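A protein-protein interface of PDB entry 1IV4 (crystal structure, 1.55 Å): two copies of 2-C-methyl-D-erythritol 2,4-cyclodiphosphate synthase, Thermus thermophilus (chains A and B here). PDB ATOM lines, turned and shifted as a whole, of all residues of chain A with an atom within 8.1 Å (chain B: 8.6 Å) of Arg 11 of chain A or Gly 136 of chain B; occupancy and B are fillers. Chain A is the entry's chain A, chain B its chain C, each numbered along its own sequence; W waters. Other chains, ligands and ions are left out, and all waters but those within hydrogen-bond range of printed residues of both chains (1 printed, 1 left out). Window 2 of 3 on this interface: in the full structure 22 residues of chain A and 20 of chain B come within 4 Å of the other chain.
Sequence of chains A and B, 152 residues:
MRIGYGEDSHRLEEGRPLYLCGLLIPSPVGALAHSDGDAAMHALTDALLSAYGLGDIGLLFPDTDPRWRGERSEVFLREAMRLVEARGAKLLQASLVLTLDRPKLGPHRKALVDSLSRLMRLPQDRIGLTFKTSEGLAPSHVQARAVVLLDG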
ATOM      1  N   ASP A   8     -10.615  25.961 -35.346  1.00  0.00           N
ATOM      2  CA  ASP A   8      -9.673  26.944 -34.791  1.00  0.00           C
ATOM      3  C   ASP A   8      -9.015  26.322 -33.571  1.00  0.00           C
ATOM      4  O   ASP A   8      -9.551  25.411 -32.950  1.00  0.00           O
ATOM      5  CB  ASP A   8     -10.334  28.271 -34.430  1.00  0.00           C
ATOM      6  CG  ASP A   8      -9.315  29.393 -34.222  1.00  0.00           C
ATOM      7  OD1 ASP A   8      -8.151  29.242 -34.656  1.00  0.00           O
ATOM      8  OD2 ASP A   8      -9.626  30.246 -33.351  1.00  0.00           O
ATOM      9  N   SER A   9      -7.836  26.811 -33.210  1.00  0.00           N
ATOM     10  CA  SER A   9      -7.260  26.445 -31.930  1.00  0.00           C
ATOM     11  C   SER A   9      -6.427  27.634 -31.427  1.00  0.00           C
ATOM     12  O   SER A   9      -5.984  28.468 -32.209  1.00  0.00           O
ATOM     13  CB  SER A   9      -6.415  25.187 -32.012  1.00  0.00           C
ATOM     14  OG  SER A   9      -5.293  25.366 -32.841  1.00  0.00           O
ATOM     15  N   HIS A  10      -6.248  27.641 -30.113  1.00  0.00           N
ATOM     16  CA  HIS A  10      -5.406  28.663 -29.510  1.00  0.00           C
ATOM     17  C   HIS A  10      -4.667  28.045 -28.325  1.00  0.00           C
ATOM     18  O   HIS A  10      -5.245  27.276 -27.582  1.00  0.00           O
ATOM     19  CB  HIS A  10      -6.207  29.878 -29.054  1.00  0.00           C
ATOM     20  CG  HIS A  10      -6.660  30.763 -30.158  1.00  0.00           C
ATOM     21  ND1 HIS A  10      -5.834  31.689 -30.755  1.00  0.00           N
ATOM     22  CD2 HIS A  10      -7.860  30.889 -30.780  1.00  0.00           C
ATOM     23  CE1 HIS A  10      -6.498  32.343 -31.697  1.00  0.00           C
ATOM     24  NE2 HIS A  10      -7.729  31.872 -31.737  1.00  0.00           N
ATOM     25  N   ARG A  11      -3.394  28.435 -28.211  1.00  0.00           N
ATOM     26  CA  ARG A  11      -2.649  28.123 -27.008  1.00  0.00           C
ATOM     27  C   ARG A  11      -3.298  28.825 -25.815  1.00  0.00           C
ATOM     28  O   ARG A  11      -3.722  29.989 -25.917  1.00  0.00           O
ATOM     29  CB  ARG A  11      -1.210  28.601 -27.168  1.00  0.00           C
ATOM     30  CG  ARG A  11      -0.191  27.946 -26.248  1.00  0.00           C
ATOM     31  CD  ARG A  11       1.219  28.186 -26.792  1.00  0.00           C
ATOM     32  NE  ARG A  11       1.681  27.048 -27.580  1.00  0.00           N
ATOM     33  CZ  ARG A  11       2.055  25.863 -27.123  1.00  0.00           C
ATOM     34  NH1 ARG A  11       2.046  25.562 -25.828  1.00  0.00           N
ATOM     35  NH2 ARG A  11       2.453  24.921 -27.974  1.00  0.00           N
ATOM     36  N   LEU A  12      -3.299  28.107 -24.706  1.00  0.00           N
ATOM     37  CA  LEU A  12      -3.822  28.671 -23.461  1.00  0.00           C
ATOM     38  C   LEU A  12      -2.708  29.135 -22.536  1.00  0.00           C
ATOM     39  O   LEU A  12      -1.679  28.472 -22.408  1.00  0.00           O
ATOM     40  CB  LEU A  12      -4.685  27.612 -22.759  1.00  0.00           C
ATOM     41  CG  LEU A  12      -6.001  27.323 -23.475  1.00  0.00           C
ATOM     42  CD1 LEU A  12      -6.696  26.131 -22.843  1.00  0.00           C
ATOM     43  CD2 LEU A  12      -6.885  28.561 -23.435  1.00  0.00           C
ATOM     44  N   GLU A  13      -2.905  30.282 -21.892  1.00  0.00           N
ATOM     45  CA  GLU A  13      -1.867  30.587 -20.884  1.00  0.00           C
ATOM     46  C   GLU A  13      -2.524  31.087 -19.619  1.00  0.00           C
ATOM     47  O   GLU A  13      -3.593  31.669 -19.615  1.00  0.00           O
ATOM     48  CB  GLU A  13      -0.843  31.553 -21.466  1.00  0.00           C
ATOM     49  CG  GLU A  13       0.199  30.794 -22.304  1.00  0.00           C
ATOM     50  CD  GLU A  13       1.085  31.779 -23.048  1.00  0.00           C
ATOM     51  OE1 GLU A  13       0.545  32.781 -23.573  1.00  0.00           O
ATOM     52  OE2 GLU A  13       2.303  31.521 -23.075  1.00  0.00           O
ATOM     53  N   GLU A  14      -1.845  30.838 -18.500  1.00  0.00           N
ATOM     54  CA  GLU A  14      -2.376  31.243 -17.217  1.00  0.00           C
ATOM     55  C   GLU A  14      -2.574  32.753 -17.145  1.00  0.00           C
ATOM     56  O   GLU A  14      -1.708  33.522 -17.565  1.00  0.00           O
ATOM     57  CB  GLU A  14      -1.398  30.748 -16.137  1.00  0.00           C
ATOM     58  CG  GLU A  14      -1.956  29.610 -15.318  1.00  0.00           C
ATOM     59  CD  GLU A  14      -1.252  28.282 -15.415  1.00  0.00           C
ATOM     60  OE1 GLU A  14      -1.935  27.266 -15.119  1.00  0.00           O
ATOM     61  OE2 GLU A  14      -0.057  28.199 -15.764  1.00  0.00           O
ATOM     62  N   ARG A  16      -4.705  34.875 -18.619  1.00  0.00           N
ATOM     63  CA  ARG A  16      -5.222  35.670 -19.741  1.00  0.00           C
ATOM     64  C   ARG A  16      -6.741  35.454 -19.721  1.00  0.00           C
ATOM     65  O   ARG A  16      -7.173  34.385 -19.251  1.00  0.00           O
ATOM     66  CB  ARG A  16      -4.600  35.280 -21.055  1.00  0.00           C
ATOM     67  CG  ARG A  16      -3.079  35.397 -21.155  1.00  0.00           C
ATOM     68  CD  ARG A  16      -2.541  34.728 -22.399  1.00  0.00           C
ATOM     69  NE  ARG A  16      -1.122  34.897 -22.647  1.00  0.00           N
ATOM     70  CZ  ARG A  16      -0.457  36.002 -22.940  1.00  0.00           C
ATOM     71  NH1 ARG A  16      -1.073  37.175 -23.039  1.00  0.00           N
ATOM     72  NH2 ARG A  16       0.862  35.970 -23.139  1.00  0.00           N
ATOM     73  N   PRO A  17      -7.547  36.403 -20.163  1.00  0.00           N
ATOM     74  CA  PRO A  17      -8.992  36.174 -20.202  1.00  0.00           C
ATOM     75  C   PRO A  17      -9.384  35.130 -21.246  1.00  0.00           C
ATOM     76  O   PRO A  17      -8.803  34.999 -22.312  1.00  0.00           O
ATOM     77  CB  PRO A  17      -9.554  37.564 -20.539  1.00  0.00           C
ATOM     78  CG  PRO A  17      -8.438  38.227 -21.288  1.00  0.00           C
ATOM     79  CD  PRO A  17      -7.169  37.751 -20.633  1.00  0.00           C
ATOM     80  N   LEU A  18     -10.410  34.332 -20.953  1.00  0.00           N
ATOM     81  CA  LEU A  18     -10.886  33.309 -21.866  1.00  0.00           C
ATOM     82  C   LEU A  18     -12.179  33.774 -22.526  1.00  0.00           C
ATOM     83  O   LEU A  18     -13.152  34.051 -21.820  1.00  0.00           O
ATOM     84  CB  LEU A  18     -11.155  32.010 -21.097  1.00  0.00           C
ATOM     85  CG  LEU A  18     -11.705  30.866 -21.975  1.00  0.00           C
ATOM     86  CD1 LEU A  18     -10.754  30.556 -23.127  1.00  0.00           C
ATOM     87  CD2 LEU A  18     -11.966  29.618 -21.152  1.00  0.00           C
ATOM     88  N   VAL A  29      -7.004  30.166 -17.152  1.00  0.00           N
ATOM     89  CA  VAL A  29      -6.260  30.250 -18.392  1.00  0.00           C
ATOM     90  C   VAL A  29      -7.099  30.866 -19.513  1.00  0.00           C
ATOM     91  O   VAL A  29      -8.328  30.794 -19.516  1.00  0.00           O
ATOM     92  CB  VAL A  29      -5.766  28.872 -18.876  1.00  0.00           C
ATOM     93  CG1 VAL A  29      -4.777  28.289 -17.879  1.00  0.00           C
ATOM     94  CG2 VAL A  29      -6.926  27.904 -19.097  1.00  0.00           C
ATOM     95  N   GLY A  30      -6.413  31.479 -20.467  1.00  0.00           N
ATOM     96  CA  GLY A  30      -7.087  32.110 -21.596  1.00  0.00           C
ATOM     97  C   GLY A  30      -6.181  32.185 -22.802  1.00  0.00           C
ATOM     98  O   GLY A  30      -4.992  31.831 -22.786  1.00  0.00           O
ATOM     99  N   ALA A  31      -6.773  32.647 -23.912  1.00  0.00           N
ATOM    100  CA  ALA A  31      -6.021  32.541 -25.153  1.00  0.00           C
ATOM    101  C   ALA A  31      -4.816  33.483 -25.127  1.00  0.00           C
ATOM    102  O   ALA A  31      -4.958  34.634 -24.708  1.00  0.00           O
ATOM    103  CB  ALA A  31      -6.898  32.819 -26.362  1.00  0.00           C
ATOM    104  N   LEU A  32      -3.716  32.900 -25.589  1.00  0.00           N
ATOM    105  CA  LEU A  32      -2.520  33.650 -25.942  1.00  0.00           C
ATOM    106  C   LEU A  32      -2.698  34.050 -27.400  1.00  0.00           C
ATOM    107  O   LEU A  32      -2.504  33.215 -28.287  1.00  0.00           O
ATOM    108  CB  LEU A  32      -1.217  32.868 -25.773  1.00  0.00           C
ATOM    109  CG  LEU A  32      -0.120  33.309 -26.751  1.00  0.00           C
ATOM    110  CD1 LEU A  32       0.742  34.397 -26.124  1.00  0.00           C
ATOM    111  CD2 LEU A  32       0.719  32.127 -27.191  1.00  0.00           C
ATOM    112  N   ALA A  33      -3.109  35.292 -27.666  1.00  0.00           N
ATOM    113  CA  ALA A  33      -3.359  35.583 -29.084  1.00  0.00           C
ATOM    114  C   ALA A  33      -3.329  37.077 -29.368  1.00  0.00           C
ATOM    115  O   ALA A  33      -3.365  37.898 -28.451  1.00  0.00           O
ATOM    116  CB  ALA A  33      -4.701  35.002 -29.515  1.00  0.00           C
ATOM    117  N   GLY A  37      -8.920  35.404 -29.234  1.00  0.00           N
ATOM    118  CA  GLY A  37      -8.675  33.982 -29.189  1.00  0.00           C
ATOM    119  C   GLY A  37      -9.935  33.161 -29.016  1.00  0.00           C
ATOM    120  O   GLY A  37      -9.880  32.048 -28.512  1.00  0.00           O
ATOM    121  N   PRO A 139      -3.422  19.648 -23.380  1.00  0.00           N
ATOM    122  CA  PRO A 139      -3.805  20.303 -22.134  1.00  0.00           C
ATOM    123  C   PRO A 139      -3.575  21.803 -22.101  1.00  0.00           C
ATOM    124  O   PRO A 139      -4.124  22.463 -21.210  1.00  0.00           O
ATOM    125  CB  PRO A 139      -2.839  19.673 -21.113  1.00  0.00           C
ATOM    126  CG  PRO A 139      -1.686  19.230 -21.934  1.00  0.00           C
ATOM    127  CD  PRO A 139      -2.237  18.774 -23.260  1.00  0.00           C
ATOM    128  N   SER A 140      -2.786  22.349 -23.013  1.00  0.00           N
ATOM    129  CA  SER A 140      -2.590  23.790 -23.019  1.00  0.00           C
ATOM    130  C   SER A 140      -3.245  24.454 -24.235  1.00  0.00           C
ATOM    131  O   SER A 140      -2.773  25.514 -24.638  1.00  0.00           O
ATOM    132  CB  SER A 140      -1.098  24.133 -22.982  1.00  0.00           C
ATOM    133  OG  SER A 140      -0.470  23.623 -21.817  1.00  0.00           O
ATOM    134  N   HIS A 141      -4.283  23.855 -24.820  1.00  0.00           N
ATOM    135  CA  HIS A 141      -4.955  24.494 -25.947  1.00  0.00           C
ATOM    136  C   HIS A 141      -6.469  24.449 -25.817  1.00  0.00           C
ATOM    137  O   HIS A 141      -6.974  23.541 -25.158  1.00  0.00           O
ATOM    138  CB  HIS A 141      -4.618  23.816 -27.283  1.00  0.00           C
ATOM    139  CG  HIS A 141      -3.187  24.040 -27.658  1.00  0.00           C
ATOM    140  ND1 HIS A 141      -2.781  24.897 -28.642  1.00  0.00           N
ATOM    141  CD2 HIS A 141      -2.058  23.487 -27.151  1.00  0.00           C
ATOM    142  CE1 HIS A 141      -1.456  24.873 -28.741  1.00  0.00           C
ATOM    143  NE2 HIS A 141      -1.001  24.030 -27.845  1.00  0.00           N
ATOM    144  N   VAL A 142      -7.130  25.391 -26.482  1.00  0.00           N
ATOM    145  CA  VAL A 142      -8.566  25.299 -26.719  1.00  0.00           C
ATOM    146  C   VAL A 142      -8.719  25.031 -28.219  1.00  0.00           C
ATOM    147  O   VAL A 142      -8.042  25.696 -29.011  1.00  0.00           O
ATOM    148  CB  VAL A 142      -9.335  26.531 -26.246  1.00  0.00           C
ATOM    149  CG1 VAL A 142      -8.836  27.856 -26.837  1.00  0.00           C
ATOM    150  CG2 VAL A 142     -10.818  26.342 -26.530  1.00  0.00           C
ATOM    151  N   GLN A 143      -9.587  24.059 -28.544  1.00  0.00           N
ATOM    152  CA  GLN A 143      -9.812  23.715 -29.941  1.00  0.00           C
ATOM    153  C   GLN A 143     -11.316  23.767 -30.207  1.00  0.00           C
ATOM    154  O   GLN A 143     -12.087  23.432 -29.301  1.00  0.00           O
ATOM    155  CB  GLN A 143      -9.312  22.327 -30.317  1.00  0.00           C
ATOM    156  CG  GLN A 143      -7.893  22.082 -29.806  1.00  0.00           C
ATOM    157  CD  GLN A 143      -7.552  20.598 -29.863  1.00  0.00           C
ATOM    158  OE1 GLN A 143      -7.424  19.933 -28.827  1.00  0.00           O
ATOM    159  NE2 GLN A 143      -7.432  20.112 -31.099  1.00  0.00           N
ATOM    160  N   THR B  99      -4.496  21.872 -41.741  1.00  0.00           N
ATOM    161  CA  THR B  99      -3.740  22.330 -40.585  1.00  0.00           C
ATOM    162  C   THR B  99      -2.253  22.070 -40.825  1.00  0.00           C
ATOM    163  O   THR B  99      -1.836  20.950 -41.045  1.00  0.00           O
ATOM    164  CB  THR B  99      -4.211  21.658 -39.286  1.00  0.00           C
ATOM    165  OG1 THR B  99      -5.617  21.872 -39.137  1.00  0.00           O
ATOM    166  CG2 THR B  99      -3.533  22.329 -38.107  1.00  0.00           C
ATOM    167  N   LEU B 100      -1.506  23.179 -40.830  1.00  0.00           N
ATOM    168  CA  LEU B 100      -0.056  23.021 -40.890  1.00  0.00           C
ATOM    169  C   LEU B 100       0.606  24.371 -40.611  1.00  0.00           C
ATOM    170  O   LEU B 100       0.062  25.421 -40.966  1.00  0.00           O
ATOM    171  CB  LEU B 100       0.414  22.448 -42.211  1.00  0.00           C
ATOM    172  CG  LEU B 100       0.243  23.368 -43.408  1.00  0.00           C
ATOM    173  CD1 LEU B 100       1.106  22.890 -44.568  1.00  0.00           C
ATOM    174  CD2 LEU B 100      -1.223  23.440 -43.803  1.00  0.00           C
ATOM    175  N   ASP B 101       1.751  24.236 -39.943  1.00  0.00           N
ATOM    176  CA  ASP B 101       2.370  25.473 -39.454  1.00  0.00           C
ATOM    177  C   ASP B 101       3.085  26.208 -40.582  1.00  0.00           C
ATOM    178  O   ASP B 101       3.078  27.428 -40.650  1.00  0.00           O
ATOM    179  CB  ASP B 101       3.384  25.163 -38.355  1.00  0.00           C
ATOM    180  CG  ASP B 101       2.830  24.561 -37.085  1.00  0.00           C
ATOM    181  OD1 ASP B 101       1.617  24.460 -36.882  1.00  0.00           O
ATOM    182  OD2 ASP B 101       3.674  24.179 -36.234  1.00  0.00           O
ATOM    183  N   THR B 133      -2.810  27.164 -38.738  1.00  0.00           N
ATOM    184  CA  THR B 133      -1.621  26.567 -38.121  1.00  0.00           C
ATOM    185  C   THR B 133      -2.078  25.662 -36.985  1.00  0.00           C
ATOM    186  O   THR B 133      -3.269  25.584 -36.704  1.00  0.00           O
ATOM    187  CB  THR B 133      -0.616  27.568 -37.526  1.00  0.00           C
ATOM    188  OG1 THR B 133      -1.228  28.244 -36.419  1.00  0.00           O
ATOM    189  CG2 THR B 133      -0.293  28.642 -38.547  1.00  0.00           C
ATOM    190  N   SER B 134      -1.115  24.996 -36.357  1.00  0.00           N
ATOM    191  CA  SER B 134      -1.478  24.065 -35.293  1.00  0.00           C
ATOM    192  C   SER B 134      -1.266  24.741 -33.938  1.00  0.00           C
ATOM    193  O   SER B 134      -1.510  24.083 -32.917  1.00  0.00           O
ATOM    194  CB  SER B 134      -0.700  22.752 -35.347  1.00  0.00           C
ATOM    195  OG  SER B 134       0.676  22.834 -35.006  1.00  0.00           O
ATOM    196  N   GLU B 135      -0.824  25.992 -34.019  1.00  0.00           N
ATOM    197  CA  GLU B 135      -0.494  26.763 -32.828  1.00  0.00           C
ATOM    198  C   GLU B 135       0.414  25.926 -31.926  1.00  0.00           C
ATOM    199  O   GLU B 135       0.230  25.904 -30.715  1.00  0.00           O
ATOM    200  CB  GLU B 135      -1.745  27.201 -32.064  1.00  0.00           C
ATOM    201  CG  GLU B 135      -2.617  28.216 -32.749  1.00  0.00           C
ATOM    202  CD  GLU B 135      -2.004  29.567 -33.027  1.00  0.00           C
ATOM    203  OE1 GLU B 135      -2.614  30.379 -33.770  1.00  0.00           O
ATOM    204  OE2 GLU B 135      -0.903  29.839 -32.504  1.00  0.00           O
ATOM    205  N   GLY B 136       1.374  25.251 -32.550  1.00  0.00           N
ATOM    206  CA  GLY B 136       2.362  24.451 -31.865  1.00  0.00           C
ATOM    207  C   GLY B 136       1.961  23.059 -31.440  1.00  0.00           C
ATOM    208  O   GLY B 136       2.787  22.339 -30.863  1.00  0.00           O
ATOM    209  N   LEU B 137       0.730  22.636 -31.682  1.00  0.00           N
ATOM    210  CA  LEU B 137       0.255  21.315 -31.252  1.00  0.00           C
ATOM    211  C   LEU B 137       0.837  20.197 -32.111  1.00  0.00           C
ATOM    212  O   LEU B 137       1.084  19.113 -31.573  1.00  0.00           O
ATOM    213  CB  LEU B 137      -1.266  21.299 -31.275  1.00  0.00           C
ATOM    214  CG  LEU B 137      -2.081  20.495 -30.277  1.00  0.00           C
ATOM    215  CD1 LEU B 137      -1.586  20.698 -28.849  1.00  0.00           C
ATOM    216  CD2 LEU B 137      -3.567  20.843 -30.376  1.00  0.00           C
ATOM    217  N   ALA B 138       1.058  20.447 -33.397  1.00  0.00           N
ATOM    218  CA  ALA B 138       1.529  19.477 -34.370  1.00  0.00           C
ATOM    219  C   ALA B 138       2.481  20.092 -35.375  1.00  0.00           C
ATOM    220  O   ALA B 138       2.178  20.155 -36.566  1.00  0.00           O
ATOM    221  CB  ALA B 138       0.331  18.871 -35.101  1.00  0.00           C
ATOM    222  N   PRO B 139       3.637  20.598 -34.944  1.00  0.00           N
ATOM    223  CA  PRO B 139       4.462  21.397 -35.856  1.00  0.00           C
ATOM    224  C   PRO B 139       5.133  20.564 -36.936  1.00  0.00           C
ATOM    225  O   PRO B 139       5.664  21.089 -37.925  1.00  0.00           O
ATOM    226  CB  PRO B 139       5.475  22.023 -34.889  1.00  0.00           C
ATOM    227  CG  PRO B 139       5.512  21.157 -33.684  1.00  0.00           C
ATOM    228  CD  PRO B 139       4.179  20.464 -33.589  1.00  0.00           C
ATOM    229  N   SER B 140       5.137  19.229 -36.786  1.00  0.00           N
ATOM    230  CA  SER B 140       5.797  18.425 -37.807  1.00  0.00           C
ATOM    231  C   SER B 140       4.818  17.574 -38.603  1.00  0.00           C
ATOM    232  O   SER B 140       5.237  16.549 -39.142  1.00  0.00           O
ATOM    233  CB  SER B 140       6.841  17.507 -37.147  1.00  0.00           C
ATOM    234  OG  SER B 140       7.929  18.291 -36.688  1.00  0.00           O
ATOM    235  N   GLN B 143      -2.304  18.057 -41.478  1.00  0.00           N
ATOM    236  CA  GLN B 143      -3.578  17.434 -41.146  1.00  0.00           C
ATOM    237  C   GLN B 143      -4.663  18.028 -42.035  1.00  0.00           C
ATOM    238  O   GLN B 143      -4.649  19.211 -42.376  1.00  0.00           O
ATOM    239  CB  GLN B 143      -3.964  17.688 -39.700  1.00  0.00           C
ATOM    240  CG  GLN B 143      -2.945  17.182 -38.688  1.00  0.00           C
ATOM    241  CD  GLN B 143      -3.286  17.687 -37.300  1.00  0.00           C
ATOM    242  OE1 GLN B 143      -2.732  18.676 -36.822  1.00  0.00           O
ATOM    243  NE2 GLN B 143      -4.225  16.983 -36.663  1.00  0.00           N
HETATM  244  O   HOH W   1      -2.297  30.639 -29.811  1.00  0.00           O
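The side-chain hydroxyl (OG1) of Thr 133 of chain B sits close to the backbone NH (N) of Glu 135 of chain B (3.3 Å).
N of Leu 32 of chain A lies within hydrogen-bond range of O of Arg 11 of chain A (2.9 Å).
The side-chain hydroxyl (OG) of Ser 134 of chain B lies within hydrogen-bond range of the backbone NH (N) of Ala 138 of chain B, 2.9 Å away.
The side-chain hydroxyl (OG) of Ser 134 of chain B is in hydrogen-bond range of the backbone NH (N) of Leu 137 of chain B (3.3 Å).
The side-chain hydroxyl (OG) of Ser 134 of chain B lies within hydrogen-bond range of the side-chain carboxylate (OD1) of Asp 101 of chain B (2.7 Å).
Hydrophobic or aromatic side chains of chain A within 4 Å of the printed part of chain B: His 141.
Along chain A the printed residues that touch a printed residue of chain B span positions 9 to 143.
Among the printed residues, no Asp or Glu carboxylate lies within 4 Å of a Lys or Arg side-chain nitrogen of the other chain.
Of chain B, only Glu 135 and Gly 136 come within 4 Å of Arg 11 of chain A.
Leu 32 of chain A touches none of the printed residues of chain B.
Printed residues of chain B within 4 Å of Gln 143 of chain A: Leu 137 (3.999 Å).
Of the printed residues of chain A, Glu 135 of chain B touches Ser 9, Arg 11 and His 141.
Gly 136 of chain B touches one residue of chain A.
Printed residues of chain A within 4 Å of Leu 137 of chain B: His 141 (3.3 Å) and Gln 143 (3.999 Å).
The nearest printed residue of chain A that does not touch Ser 134 of chain B is His 141 of chain A (4.3 Å).
Water W1 lies within hydrogen-bond range of N of Arg 11 of chain A, O of Leu 32 of chain A and OE2 of Glu 135 of chain B.
Among the printed residues, pairs that only touch across the chains: His 141 of chain A with Glu 135 of chain B (2.8 Å), His 141 of chain A with Leu 137 of chain B (3.3 Å), Ser 9 of chain A with Glu 135 of chain B (3.4 Å), Arg 11 of chain A with Glu 135 of chain B (3.6 Å), Arg 11 of chain A with Gly 136 of chain B (3.9 Å), Ser 9 of chain A with Ser 134 of chain B (3.995 Å) and Gln 143 of chain A with Leu 137 of chain B (3.999 Å).
Positions printed for both chains: 139, 140 and 143.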
